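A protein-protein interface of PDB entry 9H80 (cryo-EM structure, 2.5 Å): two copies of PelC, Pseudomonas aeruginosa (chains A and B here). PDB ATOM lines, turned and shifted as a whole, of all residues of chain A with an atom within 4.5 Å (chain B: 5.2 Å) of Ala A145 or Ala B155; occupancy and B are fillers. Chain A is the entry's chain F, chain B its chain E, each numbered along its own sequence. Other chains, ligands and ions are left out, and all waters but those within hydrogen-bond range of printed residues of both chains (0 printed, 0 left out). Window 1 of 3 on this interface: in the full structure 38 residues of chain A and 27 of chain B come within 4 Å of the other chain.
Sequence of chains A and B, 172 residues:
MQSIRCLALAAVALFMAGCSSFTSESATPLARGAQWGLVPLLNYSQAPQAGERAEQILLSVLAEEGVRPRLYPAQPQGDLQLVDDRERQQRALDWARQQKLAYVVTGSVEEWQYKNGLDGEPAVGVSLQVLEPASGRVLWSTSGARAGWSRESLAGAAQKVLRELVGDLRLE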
ATOM      1  N   CYS A  19      11.363  13.723 -27.094  1.00  0.00           N
ATOM      2  CA  CYS A  19      11.142  14.413 -25.792  1.00  0.00           C
ATOM      3  C   CYS A  19      11.205  13.413 -24.644  1.00  0.00           C
ATOM      4  O   CYS A  19      10.322  12.572 -24.503  1.00  0.00           O
ATOM      5  CB  CYS A  19       9.796  15.133 -25.794  1.00  0.00           C
ATOM      6  SG  CYS A  19       9.672  16.443 -27.028  1.00  0.00           S
ATOM      7  N   SER A  20      12.248  13.519 -23.824  1.00  0.00           N
ATOM      8  CA  SER A  20      12.514  12.562 -22.759  1.00  0.00           C
ATOM      9  C   SER A  20      12.820  13.291 -21.458  1.00  0.00           C
ATOM     10  O   SER A  20      12.968  14.516 -21.418  1.00  0.00           O
ATOM     11  CB  SER A  20      13.680  11.633 -23.122  1.00  0.00           C
ATOM     12  OG  SER A  20      13.608  11.227 -24.476  1.00  0.00           O
ATOM     13  N   SER A  21      12.915  12.510 -20.385  1.00  0.00           N
ATOM     14  CA  SER A  21      13.193  13.028 -19.053  1.00  0.00           C
ATOM     15  C   SER A  21      13.871  11.930 -18.250  1.00  0.00           C
ATOM     16  O   SER A  21      13.376  10.803 -18.210  1.00  0.00           O
ATOM     17  CB  SER A  21      11.905  13.484 -18.357  1.00  0.00           C
ATOM     18  OG  SER A  21      12.164  14.501 -17.407  1.00  0.00           O
ATOM     19  N   PHE A  22      14.998  12.260 -17.620  1.00  0.00           N
ATOM     20  CA  PHE A  22      15.774  11.293 -16.857  1.00  0.00           C
ATOM     21  C   PHE A  22      16.290  11.935 -15.579  1.00  0.00           C
ATOM     22  O   PHE A  22      16.746  13.081 -15.593  1.00  0.00           O
ATOM     23  CB  PHE A  22      16.953  10.757 -17.678  1.00  0.00           C
ATOM     24  CG  PHE A  22      16.536  10.009 -18.907  1.00  0.00           C
ATOM     25  CD1 PHE A  22      16.216   8.667 -18.837  1.00  0.00           C
ATOM     26  CD2 PHE A  22      16.456  10.648 -20.129  1.00  0.00           C
ATOM     27  CE1 PHE A  22      15.828   7.978 -19.963  1.00  0.00           C
ATOM     28  CE2 PHE A  22      16.069   9.964 -21.258  1.00  0.00           C
ATOM     29  CZ  PHE A  22      15.755   8.626 -21.176  1.00  0.00           C
ATOM     30  N   GLU A 111       4.678   3.711 -17.531  1.00  0.00           N
ATOM     31  CA  GLU A 111       3.914   3.939 -18.747  1.00  0.00           C
ATOM     32  C   GLU A 111       4.446   3.043 -19.851  1.00  0.00           C
ATOM     33  O   GLU A 111       5.661   2.947 -20.043  1.00  0.00           O
ATOM     34  CB  GLU A 111       3.992   5.406 -19.174  1.00  0.00           C
ATOM     35  CG  GLU A 111       2.999   5.789 -20.248  1.00  0.00           C
ATOM     36  CD  GLU A 111       2.806   7.284 -20.339  1.00  0.00           C
ATOM     37  OE1 GLU A 111       3.722   8.023 -19.931  1.00  0.00           O
ATOM     38  OE2 GLU A 111       1.740   7.722 -20.816  1.00  0.00           O
ATOM     39  N   VAL A 124       6.776   5.820 -23.086  1.00  0.00           N
ATOM     40  CA  VAL A 124       7.335   4.821 -22.184  1.00  0.00           C
ATOM     41  C   VAL A 124       7.877   5.532 -20.955  1.00  0.00           C
ATOM     42  O   VAL A 124       8.528   6.575 -21.073  1.00  0.00           O
ATOM     43  CB  VAL A 124       8.448   3.997 -22.860  1.00  0.00           C
ATOM     44  CG1 VAL A 124       9.044   3.007 -21.869  1.00  0.00           C
ATOM     45  CG2 VAL A 124       7.914   3.277 -24.080  1.00  0.00           C
ATOM     46  N   GLY A 125       7.604   4.966 -19.783  1.00  0.00           N
ATOM     47  CA  GLY A 125       8.187   5.437 -18.543  1.00  0.00           C
ATOM     48  C   GLY A 125       8.587   4.275 -17.661  1.00  0.00           C
ATOM     49  O   GLY A 125       7.746   3.447 -17.303  1.00  0.00           O
ATOM     50  N   SER A 143      14.775   7.181 -12.895  1.00  0.00           N
ATOM     51  CA  SER A 143      13.527   7.087 -13.639  1.00  0.00           C
ATOM     52  C   SER A 143      13.695   7.752 -14.993  1.00  0.00           C
ATOM     53  O   SER A 143      14.248   8.852 -15.090  1.00  0.00           O
ATOM     54  CB  SER A 143      12.372   7.742 -12.879  1.00  0.00           C
ATOM     55  OG  SER A 143      11.812   6.846 -11.938  1.00  0.00           O
ATOM     56  N   GLY A 144      13.220   7.075 -16.031  1.00  0.00           N
ATOM     57  CA  GLY A 144      13.281   7.603 -17.377  1.00  0.00           C
ATOM     58  C   GLY A 144      11.904   7.629 -18.002  1.00  0.00           C
ATOM     59  O   GLY A 144      11.047   6.798 -17.704  1.00  0.00           O
ATOM     60  N   ALA A 145      11.701   8.608 -18.878  1.00  0.00           N
ATOM     61  CA  ALA A 145      10.449   8.752 -19.604  1.00  0.00           C
ATOM     62  C   ALA A 145      10.748   9.305 -20.985  1.00  0.00           C
ATOM     63  O   ALA A 145      11.706  10.057 -21.170  1.00  0.00           O
ATOM     64  CB  ALA A 145       9.466   9.667 -18.864  1.00  0.00           C
ATOM     65  N   ARG A 146       9.923   8.924 -21.957  1.00  0.00           N
ATOM     66  CA  ARG A 146      10.134   9.347 -23.333  1.00  0.00           C
ATOM     67  C   ARG A 146       8.804   9.353 -24.068  1.00  0.00           C
ATOM     68  O   ARG A 146       8.005   8.429 -23.922  1.00  0.00           O
ATOM     69  CB  ARG A 146      11.131   8.426 -24.052  1.00  0.00           C
ATOM     70  CG  ARG A 146      11.204   8.595 -25.570  1.00  0.00           C
ATOM     71  CD  ARG A 146      12.224   7.656 -26.184  1.00  0.00           C
ATOM     72  NE  ARG A 146      12.373   7.882 -27.618  1.00  0.00           N
ATOM     73  CZ  ARG A 146      13.187   8.772 -28.170  1.00  0.00           C
ATOM     74  NH1 ARG A 146      13.961   9.558 -27.440  1.00  0.00           N
ATOM     75  NH2 ARG A 146      13.223   8.881 -29.495  1.00  0.00           N
ATOM     76  N   VAL A 161      14.948   4.345 -23.831  1.00  0.00           N
ATOM     77  CA  VAL A 161      14.864   4.762 -22.433  1.00  0.00           C
ATOM     78  C   VAL A 161      15.753   3.882 -21.567  1.00  0.00           C
ATOM     79  O   VAL A 161      16.498   4.370 -20.708  1.00  0.00           O
ATOM     80  CB  VAL A 161      13.405   4.735 -21.946  1.00  0.00           C
ATOM     81  CG1 VAL A 161      13.339   4.919 -20.435  1.00  0.00           C
ATOM     82  CG2 VAL A 161      12.601   5.813 -22.631  1.00  0.00           C
ATOM     83  N   ILE B  57       8.439   7.314  -9.108  1.00  0.00           N
ATOM     84  CA  ILE B  57       9.113   8.479  -9.667  1.00  0.00           C
ATOM     85  C   ILE B  57       9.603   9.394  -8.551  1.00  0.00           C
ATOM     86  O   ILE B  57      10.636  10.055  -8.693  1.00  0.00           O
ATOM     87  CB  ILE B  57       8.199   9.218 -10.662  1.00  0.00           C
ATOM     88  CG1 ILE B  57       7.768   8.282 -11.799  1.00  0.00           C
ATOM     89  CG2 ILE B  57       8.931  10.413 -11.258  1.00  0.00           C
ATOM     90  CD1 ILE B  57       6.565   8.761 -12.576  1.00  0.00           C
ATOM     91  N   TRP B 112      -3.941  12.374 -12.916  1.00  0.00           N
ATOM     92  CA  TRP B 112      -3.030  11.531 -13.683  1.00  0.00           C
ATOM     93  C   TRP B 112      -3.781  11.095 -14.945  1.00  0.00           C
ATOM     94  O   TRP B 112      -4.494  10.091 -14.966  1.00  0.00           O
ATOM     95  CB  TRP B 112      -2.568  10.333 -12.855  1.00  0.00           C
ATOM     96  CG  TRP B 112      -1.300   9.695 -13.304  1.00  0.00           C
ATOM     97  CD1 TRP B 112      -1.131   8.873 -14.376  1.00  0.00           C
ATOM     98  CD2 TRP B 112      -0.020   9.800 -12.673  1.00  0.00           C
ATOM     99  NE1 TRP B 112       0.179   8.469 -14.462  1.00  0.00           N
ATOM    100  CE2 TRP B 112       0.880   9.025 -13.426  1.00  0.00           C
ATOM    101  CE3 TRP B 112       0.452  10.480 -11.548  1.00  0.00           C
ATOM    102  CZ2 TRP B 112       2.225   8.911 -13.089  1.00  0.00           C
ATOM    103  CZ3 TRP B 112       1.784  10.367 -11.218  1.00  0.00           C
ATOM    104  CH2 TRP B 112       2.656   9.586 -11.984  1.00  0.00           C
ATOM    105  N   SER B 153       5.149  12.572 -22.312  1.00  0.00           N
ATOM    106  CA  SER B 153       4.554  11.425 -21.651  1.00  0.00           C
ATOM    107  C   SER B 153       4.006  11.820 -20.283  1.00  0.00           C
ATOM    108  O   SER B 153       4.401  12.827 -19.691  1.00  0.00           O
ATOM    109  CB  SER B 153       5.584  10.306 -21.498  1.00  0.00           C
ATOM    110  OG  SER B 153       6.826  10.822 -21.055  1.00  0.00           O
ATOM    111  N   LEU B 154       3.071  11.007 -19.784  1.00  0.00           N
ATOM    112  CA  LEU B 154       2.569  11.211 -18.430  1.00  0.00           C
ATOM    113  C   LEU B 154       3.684  11.045 -17.409  1.00  0.00           C
ATOM    114  O   LEU B 154       3.771  11.807 -16.440  1.00  0.00           O
ATOM    115  CB  LEU B 154       1.433  10.232 -18.132  1.00  0.00           C
ATOM    116  CG  LEU B 154       0.006  10.773 -18.216  1.00  0.00           C
ATOM    117  CD1 LEU B 154      -0.990   9.630 -18.199  1.00  0.00           C
ATOM    118  CD2 LEU B 154      -0.273  11.737 -17.079  1.00  0.00           C
ATOM    119  N   ALA B 155       4.546  10.047 -17.613  1.00  0.00           N
ATOM    120  CA  ALA B 155       5.656   9.823 -16.696  1.00  0.00           C
ATOM    121  C   ALA B 155       6.607  11.012 -16.682  1.00  0.00           C
ATOM    122  O   ALA B 155       7.106  11.398 -15.619  1.00  0.00           O
ATOM    123  CB  ALA B 155       6.398   8.544 -17.079  1.00  0.00           C
ATOM    124  N   GLY B 156       6.867  11.610 -17.844  1.00  0.00           N
ATOM    125  CA  GLY B 156       7.741  12.770 -17.884  1.00  0.00           C
ATOM    126  C   GLY B 156       7.155  13.972 -17.169  1.00  0.00           C
ATOM    127  O   GLY B 156       7.860  14.684 -16.447  1.00  0.00           O
ATOM    128  N   ALA B 157       5.857  14.219 -17.360  1.00  0.00           N
ATOM    129  CA  ALA B 157       5.204  15.318 -16.657  1.00  0.00           C
ATOM    130  C   ALA B 157       5.223  15.090 -15.153  1.00  0.00           C
ATOM    131  O   ALA B 157       5.481  16.020 -14.377  1.00  0.00           O
ATOM    132  CB  ALA B 157       3.771  15.482 -17.158  1.00  0.00           C
ATOM    133  N   ALA B 158       4.950  13.857 -14.722  1.00  0.00           N
ATOM    134  CA  ALA B 158       5.004  13.545 -13.299  1.00  0.00           C
ATOM    135  C   ALA B 158       6.410  13.742 -12.755  1.00  0.00           C
ATOM    136  O   ALA B 158       6.590  14.237 -11.636  1.00  0.00           O
ATOM    137  CB  ALA B 158       4.532  12.115 -13.060  1.00  0.00           C
ATOM    138  N   GLN B 159       7.422  13.356 -13.533  1.00  0.00           N
ATOM    139  CA  GLN B 159       8.802  13.550 -13.111  1.00  0.00           C
ATOM    140  C   GLN B 159       9.127  15.028 -12.950  1.00  0.00           C
ATOM    141  O   GLN B 159       9.771  15.420 -11.973  1.00  0.00           O
ATOM    142  CB  GLN B 159       9.743  12.905 -14.122  1.00  0.00           C
ATOM    143  CG  GLN B 159      11.125  12.613 -13.587  1.00  0.00           C
ATOM    144  CD  GLN B 159      11.991  11.896 -14.598  1.00  0.00           C
ATOM    145  OE1 GLN B 159      13.035  12.401 -15.001  1.00  0.00           O
ATOM    146  NE2 GLN B 159      11.558  10.714 -15.017  1.00  0.00           N
ATOM    147  N   LYS B 160       8.691  15.861 -13.895  1.00  0.00           N
ATOM    148  CA  LYS B 160       8.943  17.296 -13.777  1.00  0.00           C
ATOM    149  C   LYS B 160       8.245  17.885 -12.556  1.00  0.00           C
ATOM    150  O   LYS B 160       8.839  18.680 -11.813  1.00  0.00           O
ATOM    151  CB  LYS B 160       8.487  18.013 -15.049  1.00  0.00           C
ATOM    152  CG  LYS B 160       9.320  17.689 -16.270  1.00  0.00           C
ATOM    153  CD  LYS B 160       8.861  18.479 -17.481  1.00  0.00           C
ATOM    154  CE  LYS B 160       9.576  18.030 -18.739  1.00  0.00           C
ATOM    155  NZ  LYS B 160       9.237  18.879 -19.911  1.00  0.00           N
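The backbone carbonyl oxygen (O) of Ser A21 is in hydrogen-bond range of the backbone NH (N) of Ala A145 (2.8 Å). O of Val A124 sits at hydrogen-bond distance from N of Arg A146, at 2.9 Å. The side-chain hydroxyl (OG) of Ser A20 sits at hydrogen-bond distance from the guanidinium group (NH1) of Arg A146 (3.4 Å). OG of Ser B153 lies within hydrogen-bond range of N of Gly B156, 3.3 Å away. The backbone carbonyl oxygen (O) of Glu A111 is in hydrogen-bond range of the backbone NH (N) of Gly A125.
Of the 12 printed residues of chain A, 7 touch a printed residue of chain B.
The backbone NH (N) of Ala B155 lies within hydrogen-bond range of the side-chain carboxylate (OE1) of Glu A111. OE1 of Gln B159 is in hydrogen-bond range of N of Phe A22 (3.3 Å). OE1 of Gln B159 is in hydrogen-bond range of OG of Ser A21 (3.3 Å). The side-chain amide nitrogen (NE2) of Gln B159 lies within hydrogen-bond range of the backbone carbonyl oxygen (O) of Ser A143. OE1 of Glu A111 lies within hydrogen-bond range of N of Leu B154, 3.1 Å away.
Among the printed residues, merely in contact across the chains: Glu A111 with Ser B153 (3.3 Å), Gly A125 with Ala B155 (3.9 Å), Ser A143 with Ile B57 (3.9 Å), Ala A145 with Ser B153 (3.6 Å), Ala A145 with Ala B155 (3.7 Å), Ala A145 with Gly B156 (3.4 Å) and Arg A146 with Ser B153 (3.7 Å).
Cys A19 touches none of the printed residues of chain B. Of the printed residues of chain B, Phe A22 touches Gln B159. Printed residues of chain B within 4 Å of Gly A125: Ala B155. Of the printed residues of chain B, Ser A143 touches Ile B57 (3.9 Å) and Gln B159 (3.3 Å). Ala A145 touches three residues of chain B. Printed residues of chain B within 4 Å of Arg A146: Ser B153 (3.7 Å). Of the printed residues of chain A, Ser B153 touches Glu A111, Ala A145 and Arg A146. Ala B155 touches just these residues of chain A: Glu A111 (3.2 Å), Gly A125 (3.9 Å) and Ala A145 (3.7 Å). Lys B160 touches none of the printed residues of chain A. The nearest printed residue of chain A that does not touch Gly B156 is Ser A21 (4.3 Å).
No position is printed for both chains.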
